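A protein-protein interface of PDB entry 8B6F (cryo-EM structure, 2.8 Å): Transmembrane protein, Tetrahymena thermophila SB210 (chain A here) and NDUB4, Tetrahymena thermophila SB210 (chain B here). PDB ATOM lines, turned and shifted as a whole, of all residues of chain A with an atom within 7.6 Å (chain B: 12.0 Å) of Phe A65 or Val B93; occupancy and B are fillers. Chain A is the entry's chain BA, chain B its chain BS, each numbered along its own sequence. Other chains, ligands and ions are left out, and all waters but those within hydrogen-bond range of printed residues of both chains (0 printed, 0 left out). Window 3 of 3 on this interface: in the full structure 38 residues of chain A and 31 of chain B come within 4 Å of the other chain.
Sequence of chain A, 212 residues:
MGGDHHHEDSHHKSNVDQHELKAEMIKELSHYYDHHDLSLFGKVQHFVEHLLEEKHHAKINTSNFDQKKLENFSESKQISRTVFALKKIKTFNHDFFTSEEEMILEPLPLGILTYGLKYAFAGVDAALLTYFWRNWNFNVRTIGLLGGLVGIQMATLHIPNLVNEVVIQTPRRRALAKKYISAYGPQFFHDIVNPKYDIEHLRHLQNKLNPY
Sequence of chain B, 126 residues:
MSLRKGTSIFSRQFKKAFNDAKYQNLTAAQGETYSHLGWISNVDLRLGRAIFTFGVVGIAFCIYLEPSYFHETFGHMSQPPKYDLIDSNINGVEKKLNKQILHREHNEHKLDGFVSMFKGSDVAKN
NH2 of Arg A81 lies within salt-bridge range of OE2 of Glu B94 (3.7 Å).
The side-chain amide oxygen (OD1) of Asn B98 sits close to the backbone carbonyl oxygen (O) of Val A193, 3.2 Å away.
The side-chain carboxylate (OE2) of Glu B94 lies close to the backbone carbonyl oxygen (O) of Val A193.
The backbone NH (N) of Asn A194 sits close to the side-chain carboxylate (OE2) of Glu B94, 3.4 Å away.
ND2 of Asn B98 sits at hydrogen-bond distance from O of Glu B94, 2.5 Å away.
The backbone NH of Lys A196 lies within hydrogen-bond range of the side-chain amide oxygen of Asn A194, 3.0 Å away.
The backbone carbonyl oxygen (O) of Asp A66 sits at hydrogen-bond distance from the side-chain amide nitrogen (ND2) of Asn A194, 3.0 Å away.
Phe A65 touches Val B93.
Phe A65 touches Glu B94 (CE1 to OE1, 2.8 Å).
CD1 of Ile B90 touches CG1 of Val A193, at 3.4 Å.
OE1 of Glu B94 touches CD of Pro A195 (3.0 Å).
CG of Pro A195 touches CD1 of Leu B97, 3.8 Å away.
Pro A195 touches Ile B101.
No residue of chain B comes within 4 Å of Thr A62.
No residue of chain B comes within 4 Å of Ser A63.
No residue of chain B comes within 4 Å of Asn A64.
Printed residues of chain B within 4 Å of Phe A65: Val B93 (3.6 Å) and Glu B94 (2.8 Å).
Asp A66 touches none of the printed residues of chain B.
No residue of chain B comes within 4 Å of Lys A68.
Printed residues of chain B within 4 Å of Arg A81: Glu B94 (3.7 Å).
Printed residues of chain B within 4 Å of Val A193: Ile B90, Glu B94 and Asn B98.
Of chain B, only Glu B94, Leu B97 and Ile B101 come within 4 Å of Pro A195.
Asn B89 touches none of the printed residues of chain A.
Printed residues of chain A within 4 Å of Ile B90: Val A193.
Gly B92 touches none of the printed residues of chain A.
Val B93 touches just one residue of chain A: Phe A65.
Printed residues of chain A within 4 Å of Glu B94: Phe A65, Arg A81, Val A193, Asn A194 and Pro A195.
Of the printed residues of chain A, Leu B97 touches Pro A195 (3.8 Å).
The nearest printed residue of chain A that does not touch Glu B94 is Gln A67 (6.1 Å).
Of the 13 printed residues of chain A, 5 touch a printed residue of chain B.
Hydrophobic or aromatic side chains of chain B that line the printed part of chain A: Ile B90, Val B93, Leu B97 and Ile B101.
Among the printed residues, 10 pairs touch across the chains.
Among the printed residues, Asp or Glu carboxylates within 4 Å of a Lys or Arg side-chain nitrogen of the other chain: Arg A81 with Glu B94 (3.7 Å).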
ATOM      1  N   ASN A  61      -8.898  30.311   6.091  1.00  0.00           N
ATOM      2  CA  ASN A  61      -8.259  28.999   6.054  1.00  0.00           C
ATOM      3  C   ASN A  61      -8.292  28.402   7.455  1.00  0.00           C
ATOM      4  O   ASN A  61      -7.535  28.822   8.337  1.00  0.00           O
ATOM      5  CB  ASN A  61      -6.829  29.108   5.534  1.00  0.00           C
ATOM      6  CG  ASN A  61      -6.764  29.642   4.117  1.00  0.00           C
ATOM      7  OD1 ASN A  61      -6.088  30.634   3.845  1.00  0.00           O
ATOM      8  ND2 ASN A  61      -7.471  28.985   3.203  1.00  0.00           N
ATOM      9  N   THR A  62      -9.170  27.420   7.660  1.00  0.00           N
ATOM     10  CA  THR A  62      -9.333  26.762   8.949  1.00  0.00           C
ATOM     11  C   THR A  62      -8.799  25.335   8.934  1.00  0.00           C
ATOM     12  O   THR A  62      -9.214  24.511   9.754  1.00  0.00           O
ATOM     13  CB  THR A  62     -10.805  26.766   9.365  1.00  0.00           C
ATOM     14  OG1 THR A  62     -11.590  26.082   8.378  1.00  0.00           O
ATOM     15  CG2 THR A  62     -11.315  28.190   9.518  1.00  0.00           C
ATOM     16  N   SER A  63      -7.888  25.029   8.012  1.00  0.00           N
ATOM     17  CA  SER A  63      -7.322  23.696   7.874  1.00  0.00           C
ATOM     18  C   SER A  63      -5.994  23.541   8.600  1.00  0.00           C
ATOM     19  O   SER A  63      -5.377  22.475   8.511  1.00  0.00           O
ATOM     20  CB  SER A  63      -7.137  23.355   6.391  1.00  0.00           C
ATOM     21  OG  SER A  63      -8.380  23.353   5.708  1.00  0.00           O
ATOM     22  N   ASN A  64      -5.535  24.571   9.310  1.00  0.00           N
ATOM     23  CA  ASN A  64      -4.279  24.516  10.047  1.00  0.00           C
ATOM     24  C   ASN A  64      -4.476  24.260  11.533  1.00  0.00           C
ATOM     25  O   ASN A  64      -3.703  23.506  12.133  1.00  0.00           O
ATOM     26  CB  ASN A  64      -3.500  25.822   9.860  1.00  0.00           C
ATOM     27  CG  ASN A  64      -3.107  26.065   8.417  1.00  0.00           C
ATOM     28  OD1 ASN A  64      -2.942  25.126   7.639  1.00  0.00           O
ATOM     29  ND2 ASN A  64      -2.950  27.334   8.054  1.00  0.00           N
ATOM     30  N   PHE A  65      -5.488  24.869  12.144  1.00  0.00           N
ATOM     31  CA  PHE A  65      -5.822  24.621  13.544  1.00  0.00           C
ATOM     32  C   PHE A  65      -6.825  23.474  13.589  1.00  0.00           C
ATOM     33  O   PHE A  65      -7.977  23.636  13.175  1.00  0.00           O
ATOM     34  CB  PHE A  65      -6.388  25.879  14.196  1.00  0.00           C
ATOM     35  CG  PHE A  65      -6.746  25.703  15.643  1.00  0.00           C
ATOM     36  CD1 PHE A  65      -7.987  25.208  16.011  1.00  0.00           C
ATOM     37  CD2 PHE A  65      -5.841  26.041  16.638  1.00  0.00           C
ATOM     38  CE1 PHE A  65      -8.314  25.046  17.344  1.00  0.00           C
ATOM     39  CE2 PHE A  65      -6.163  25.883  17.972  1.00  0.00           C
ATOM     40  CZ  PHE A  65      -7.402  25.384  18.326  1.00  0.00           C
ATOM     41  N   ASP A  66      -6.393  22.317  14.091  1.00  0.00           N
ATOM     42  CA  ASP A  66      -7.237  21.126  14.009  1.00  0.00           C
ATOM     43  C   ASP A  66      -8.277  21.097  15.125  1.00  0.00           C
ATOM     44  O   ASP A  66      -9.481  21.198  14.869  1.00  0.00           O
ATOM     45  CB  ASP A  66      -6.362  19.869  14.041  1.00  0.00           C
ATOM     46  CG  ASP A  66      -7.150  18.603  13.763  1.00  0.00           C
ATOM     47  OD1 ASP A  66      -8.370  18.701  13.517  1.00  0.00           O
ATOM     48  OD2 ASP A  66      -6.547  17.509  13.787  1.00  0.00           O
ATOM     49  N   GLN A  67      -7.831  20.977  16.374  1.00  0.00           N
ATOM     50  CA  GLN A  67      -8.746  20.904  17.509  1.00  0.00           C
ATOM     51  C   GLN A  67      -7.919  20.779  18.782  1.00  0.00           C
ATOM     52  O   GLN A  67      -6.694  20.634  18.743  1.00  0.00           O
ATOM     53  CB  GLN A  67      -9.723  19.728  17.386  1.00  0.00           C
ATOM     54  CG  GLN A  67     -11.012  19.905  18.179  1.00  0.00           C
ATOM     55  CD  GLN A  67     -12.052  18.858  17.836  1.00  0.00           C
ATOM     56  OE1 GLN A  67     -11.725  17.781  17.339  1.00  0.00           O
ATOM     57  NE2 GLN A  67     -13.317  19.174  18.093  1.00  0.00           N
ATOM     58  N   LYS A  68      -8.612  20.841  19.918  1.00  0.00           N
ATOM     59  CA  LYS A  68      -8.063  20.470  21.213  1.00  0.00           C
ATOM     60  C   LYS A  68      -8.973  19.430  21.849  1.00  0.00           C
ATOM     61  O   LYS A  68     -10.199  19.518  21.737  1.00  0.00           O
ATOM     62  CB  LYS A  68      -7.926  21.684  22.142  1.00  0.00           C
ATOM     63  CG  LYS A  68      -6.657  22.492  21.920  1.00  0.00           C
ATOM     64  CD  LYS A  68      -6.477  23.550  23.000  1.00  0.00           C
ATOM     65  CE  LYS A  68      -5.166  24.304  22.832  1.00  0.00           C
ATOM     66  NZ  LYS A  68      -3.979  23.413  22.957  1.00  0.00           N
ATOM     67  N   ARG A  81     -16.384  28.076  27.074  1.00  0.00           N
ATOM     68  CA  ARG A  81     -16.477  27.772  25.651  1.00  0.00           C
ATOM     69  C   ARG A  81     -17.914  27.515  25.228  1.00  0.00           C
ATOM     70  O   ARG A  81     -18.291  27.824  24.093  1.00  0.00           O
ATOM     71  CB  ARG A  81     -15.591  26.572  25.323  1.00  0.00           C
ATOM     72  CG  ARG A  81     -14.109  26.846  25.516  1.00  0.00           C
ATOM     73  CD  ARG A  81     -13.284  25.576  25.430  1.00  0.00           C
ATOM     74  NE  ARG A  81     -13.270  25.018  24.083  1.00  0.00           N
ATOM     75  CZ  ARG A  81     -12.438  25.392  23.120  1.00  0.00           C
ATOM     76  NH1 ARG A  81     -11.540  26.343  23.311  1.00  0.00           N
ATOM     77  NH2 ARG A  81     -12.506  24.791  21.935  1.00  0.00           N
ATOM     78  N   VAL A 193     -17.803  25.400  18.873  1.00  0.00           N
ATOM     79  CA  VAL A 193     -16.673  26.286  19.140  1.00  0.00           C
ATOM     80  C   VAL A 193     -15.573  26.062  18.114  1.00  0.00           C
ATOM     81  O   VAL A 193     -14.926  27.012  17.657  1.00  0.00           O
ATOM     82  CB  VAL A 193     -16.155  26.077  20.575  1.00  0.00           C
ATOM     83  CG1 VAL A 193     -14.832  26.791  20.785  1.00  0.00           C
ATOM     84  CG2 VAL A 193     -17.174  26.549  21.580  1.00  0.00           C
ATOM     85  N   ASN A 194     -15.340  24.811  17.737  1.00  0.00           N
ATOM     86  CA  ASN A 194     -14.334  24.519  16.729  1.00  0.00           C
ATOM     87  C   ASN A 194     -14.678  25.249  15.433  1.00  0.00           C
ATOM     88  O   ASN A 194     -15.812  25.135  14.948  1.00  0.00           O
ATOM     89  CB  ASN A 194     -14.246  23.015  16.483  1.00  0.00           C
ATOM     90  CG  ASN A 194     -13.152  22.651  15.500  1.00  0.00           C
ATOM     91  OD1 ASN A 194     -13.392  22.540  14.300  1.00  0.00           O
ATOM     92  ND2 ASN A 194     -11.939  22.467  16.009  1.00  0.00           N
ATOM     93  N   PRO A 195     -13.744  25.999  14.843  1.00  0.00           N
ATOM     94  CA  PRO A 195     -14.091  26.801  13.658  1.00  0.00           C
ATOM     95  C   PRO A 195     -14.487  25.979  12.446  1.00  0.00           C
ATOM     96  O   PRO A 195     -15.117  26.525  11.531  1.00  0.00           O
ATOM     97  CB  PRO A 195     -12.811  27.608  13.393  1.00  0.00           C
ATOM     98  CG  PRO A 195     -11.725  26.811  14.016  1.00  0.00           C
ATOM     99  CD  PRO A 195     -12.333  26.172  15.225  1.00  0.00           C
ATOM    100  N   LYS A 196     -14.142  24.692  12.396  1.00  0.00           N
ATOM    101  CA  LYS A 196     -14.489  23.882  11.234  1.00  0.00           C
ATOM    102  C   LYS A 196     -15.976  23.565  11.162  1.00  0.00           C
ATOM    103  O   LYS A 196     -16.423  23.011  10.152  1.00  0.00           O
ATOM    104  CB  LYS A 196     -13.689  22.579  11.238  1.00  0.00           C
ATOM    105  CG  LYS A 196     -12.182  22.782  11.247  1.00  0.00           C
ATOM    106  CD  LYS A 196     -11.445  21.455  11.152  1.00  0.00           C
ATOM    107  CE  LYS A 196      -9.939  21.662  11.180  1.00  0.00           C
ATOM    108  NZ  LYS A 196      -9.195  20.375  11.116  1.00  0.00           N
ATOM    109  N   ASP B  87     -16.180  37.032  23.941  1.00  0.00           N
ATOM    110  CA  ASP B  87     -15.077  36.590  23.097  1.00  0.00           C
ATOM    111  C   ASP B  87     -13.809  36.308  23.893  1.00  0.00           C
ATOM    112  O   ASP B  87     -12.954  35.551  23.422  1.00  0.00           O
ATOM    113  CB  ASP B  87     -14.794  37.638  22.018  1.00  0.00           C
ATOM    114  CG  ASP B  87     -14.520  39.013  22.598  1.00  0.00           C
ATOM    115  OD1 ASP B  87     -14.557  39.158  23.838  1.00  0.00           O
ATOM    116  OD2 ASP B  87     -14.268  39.953  21.814  1.00  0.00           O
ATOM    117  N   SER B  88     -13.665  36.894  25.082  1.00  0.00           N
ATOM    118  CA  SER B  88     -12.466  36.680  25.884  1.00  0.00           C
ATOM    119  C   SER B  88     -12.362  35.259  26.422  1.00  0.00           C
ATOM    120  O   SER B  88     -11.292  34.878  26.907  1.00  0.00           O
ATOM    121  CB  SER B  88     -12.426  37.674  27.047  1.00  0.00           C
ATOM    122  OG  SER B  88     -13.537  37.501  27.910  1.00  0.00           O
ATOM    123  N   ASN B  89     -13.438  34.473  26.352  1.00  0.00           N
ATOM    124  CA  ASN B  89     -13.389  33.107  26.862  1.00  0.00           C
ATOM    125  C   ASN B  89     -12.382  32.264  26.091  1.00  0.00           C
ATOM    126  O   ASN B  89     -11.654  31.457  26.681  1.00  0.00           O
ATOM    127  CB  ASN B  89     -14.777  32.473  26.794  1.00  0.00           C
ATOM    128  CG  ASN B  89     -15.766  33.132  27.733  1.00  0.00           C
ATOM    129  OD1 ASN B  89     -15.382  33.733  28.734  1.00  0.00           O
ATOM    130  ND2 ASN B  89     -17.050  33.017  27.415  1.00  0.00           N
ATOM    131  N   ILE B  90     -12.330  32.428  24.779  1.00  0.00           N
ATOM    132  CA  ILE B  90     -11.420  31.671  23.928  1.00  0.00           C
ATOM    133  C   ILE B  90     -10.150  32.482  23.724  1.00  0.00           C
ATOM    134  O   ILE B  90     -10.158  33.715  23.785  1.00  0.00           O
ATOM    135  CB  ILE B  90     -12.099  31.327  22.587  1.00  0.00           C
ATOM    136  CG1 ILE B  90     -13.328  30.454  22.845  1.00  0.00           C
ATOM    137  CG2 ILE B  90     -11.119  30.633  21.649  1.00  0.00           C
ATOM    138  CD1 ILE B  90     -14.077  30.055  21.603  1.00  0.00           C
ATOM    139  N   ASN B  91      -9.041  31.784  23.486  1.00  0.00           N
ATOM    140  CA  ASN B  91      -7.749  32.425  23.290  1.00  0.00           C
ATOM    141  C   ASN B  91      -6.978  31.710  22.191  1.00  0.00           C
ATOM    142  O   ASN B  91      -7.109  30.498  22.004  1.00  0.00           O
ATOM    143  CB  ASN B  91      -6.928  32.424  24.586  1.00  0.00           C
ATOM    144  CG  ASN B  91      -5.542  33.003  24.395  1.00  0.00           C
ATOM    145  OD1 ASN B  91      -5.302  33.779  23.469  1.00  0.00           O
ATOM    146  ND2 ASN B  91      -4.618  32.628  25.272  1.00  0.00           N
ATOM    147  N   GLY B  92      -6.168  32.479  21.464  1.00  0.00           N
ATOM    148  CA  GLY B  92      -5.263  31.920  20.478  1.00  0.00           C
ATOM    149  C   GLY B  92      -5.825  31.859  19.074  1.00  0.00           C
ATOM    150  O   GLY B  92      -6.645  32.695  18.684  1.00  0.00           O
ATOM    151  N   VAL B  93      -5.381  30.865  18.303  1.00  0.00           N
ATOM    152  CA  VAL B  93      -5.852  30.711  16.928  1.00  0.00           C
ATOM    153  C   VAL B  93      -7.354  30.473  16.910  1.00  0.00           C
ATOM    154  O   VAL B  93      -8.064  30.946  16.015  1.00  0.00           O
ATOM    155  CB  VAL B  93      -5.087  29.575  16.223  1.00  0.00           C
ATOM    156  CG1 VAL B  93      -5.645  29.337  14.826  1.00  0.00           C
ATOM    157  CG2 VAL B  93      -3.604  29.896  16.153  1.00  0.00           C
ATOM    158  N   GLU B  94      -7.862  29.731  17.895  1.00  0.00           N
ATOM    159  CA  GLU B  94      -9.303  29.543  18.011  1.00  0.00           C
ATOM    160  C   GLU B  94     -10.014  30.888  18.077  1.00  0.00           C
ATOM    161  O   GLU B  94     -10.967  31.138  17.330  1.00  0.00           O
ATOM    162  CB  GLU B  94      -9.613  28.703  19.250  1.00  0.00           C
ATOM    163  CG  GLU B  94     -11.058  28.253  19.359  1.00  0.00           C
ATOM    164  CD  GLU B  94     -11.366  27.091  18.445  1.00  0.00           C
ATOM    165  OE1 GLU B  94     -10.524  26.781  17.580  1.00  0.00           O
ATOM    166  OE2 GLU B  94     -12.446  26.484  18.590  1.00  0.00           O
ATOM    167  N   LYS B  95      -9.565  31.769  18.971  1.00  0.00           N
ATOM    168  CA  LYS B  95     -10.189  33.082  19.093  1.00  0.00           C
ATOM    169  C   LYS B  95     -10.074  33.869  17.794  1.00  0.00           C
ATOM    170  O   LYS B  95     -11.045  34.491  17.348  1.00  0.00           O
ATOM    171  CB  LYS B  95      -9.549  33.857  20.245  1.00  0.00           C
ATOM    172  CG  LYS B  95     -10.124  35.249  20.460  1.00  0.00           C
ATOM    173  CD  LYS B  95      -9.349  36.000  21.532  1.00  0.00           C
ATOM    174  CE  LYS B  95      -9.904  37.398  21.735  1.00  0.00           C
ATOM    175  NZ  LYS B  95      -9.139  38.149  22.768  1.00  0.00           N
ATOM    176  N   LYS B  96      -8.895  33.855  17.170  1.00  0.00           N
ATOM    177  CA  LYS B  96      -8.700  34.619  15.942  1.00  0.00           C
ATOM    178  C   LYS B  96      -9.651  34.154  14.847  1.00  0.00           C
ATOM    179  O   LYS B  96     -10.342  34.966  14.222  1.00  0.00           O
ATOM    180  CB  LYS B  96      -7.248  34.493  15.478  1.00  0.00           C
ATOM    181  CG  LYS B  96      -6.923  35.291  14.220  1.00  0.00           C
ATOM    182  CD  LYS B  96      -5.511  35.007  13.719  1.00  0.00           C
ATOM    183  CE  LYS B  96      -4.449  35.389  14.741  1.00  0.00           C
ATOM    184  NZ  LYS B  96      -4.568  36.805  15.192  1.00  0.00           N
ATOM    185  N   LEU B  97      -9.704  32.843  14.603  1.00  0.00           N
ATOM    186  CA  LEU B  97     -10.556  32.325  13.537  1.00  0.00           C
ATOM    187  C   LEU B  97     -12.027  32.602  13.820  1.00  0.00           C
ATOM    188  O   LEU B  97     -12.775  33.001  12.920  1.00  0.00           O
ATOM    189  CB  LEU B  97     -10.319  30.826  13.361  1.00  0.00           C
ATOM    190  CG  LEU B  97      -8.914  30.414  12.917  1.00  0.00           C
ATOM    191  CD1 LEU B  97      -8.823  28.903  12.790  1.00  0.00           C
ATOM    192  CD2 LEU B  97      -8.528  31.083  11.604  1.00  0.00           C
ATOM    193  N   ASN B  98     -12.461  32.399  15.063  1.00  0.00           N
ATOM    194  CA  ASN B  98     -13.860  32.642  15.396  1.00  0.00           C
ATOM    195  C   ASN B  98     -14.209  34.117  15.258  1.00  0.00           C
ATOM    196  O   ASN B  98     -15.298  34.461  14.785  1.00  0.00           O
ATOM    197  CB  ASN B  98     -14.157  32.145  16.809  1.00  0.00           C
ATOM    198  CG  ASN B  98     -14.255  30.634  16.882  1.00  0.00           C
ATOM    199  OD1 ASN B  98     -15.348  30.071  16.860  1.00  0.00           O
ATOM    200  ND2 ASN B  98     -13.110  29.970  16.967  1.00  0.00           N
ATOM    201  N   LYS B  99     -13.298  35.006  15.659  1.00  0.00           N
ATOM    202  CA  LYS B  99     -13.555  36.433  15.503  1.00  0.00           C
ATOM    203  C   LYS B  99     -13.676  36.808  14.032  1.00  0.00           C
ATOM    204  O   LYS B  99     -14.561  37.583  13.652  1.00  0.00           O
ATOM    205  CB  LYS B  99     -12.442  37.236  16.175  1.00  0.00           C
ATOM    206  CG  LYS B  99     -12.680  38.739  16.189  1.00  0.00           C
ATOM    207  CD  LYS B  99     -11.484  39.492  16.763  1.00  0.00           C
ATOM    208  CE  LYS B  99     -11.223  39.135  18.220  1.00  0.00           C
ATOM    209  NZ  LYS B  99     -12.412  39.377  19.084  1.00  0.00           N
ATOM    210  N   GLN B 100     -12.793  36.271  13.186  1.00  0.00           N
ATOM    211  CA  GLN B 100     -12.889  36.547  11.756  1.00  0.00           C
ATOM    212  C   GLN B 100     -14.197  36.020  11.183  1.00  0.00           C
ATOM    213  O   GLN B 100     -14.841  36.689  10.366  1.00  0.00           O
ATOM    214  CB  GLN B 100     -11.697  35.936  11.019  1.00  0.00           C
ATOM    215  CG  GLN B 100     -10.370  36.600  11.347  1.00  0.00           C
ATOM    216  CD  GLN B 100      -9.218  36.009  10.561  1.00  0.00           C
ATOM    217  OE1 GLN B 100      -9.399  35.080   9.776  1.00  0.00           O
ATOM    218  NE2 GLN B 100      -8.022  36.547  10.769  1.00  0.00           N
ATOM    219  N   ILE B 101     -14.608  34.821  11.598  1.00  0.00           N
ATOM    220  CA  ILE B 101     -15.865  34.258  11.112  1.00  0.00           C
ATOM    221  C   ILE B 101     -17.037  35.136  11.533  1.00  0.00           C
ATOM    222  O   ILE B 101     -17.956  35.388  10.746  1.00  0.00           O
ATOM    223  CB  ILE B 101     -16.027  32.810  11.612  1.00  0.00           C
ATOM    224  CG1 ILE B 101     -15.003  31.900  10.928  1.00  0.00           C
ATOM    225  CG2 ILE B 101     -17.443  32.302  11.356  1.00  0.00           C
ATOM    226  CD1 ILE B 101     -14.933  30.500  11.506  1.00  0.00           C
ATOM    227  N   LEU B 102     -17.026  35.614  12.778  1.00  0.00           N
ATOM    228  CA  LEU B 102     -18.113  36.467  13.247  1.00  0.00           C
ATOM    229  C   LEU B 102     -18.152  37.783  12.480  1.00  0.00           C
ATOM    230  O   LEU B 102     -19.231  38.272  12.129  1.00  0.00           O
ATOM    231  CB  LEU B 102     -17.972  36.728  14.747  1.00  0.00           C
ATOM    232  CG  LEU B 102     -18.199  35.530  15.674  1.00  0.00           C
ATOM    233  CD1 LEU B 102     -17.950  35.930  17.117  1.00  0.00           C
ATOM    234  CD2 LEU B 102     -19.599  34.959  15.518  1.00  0.00           C
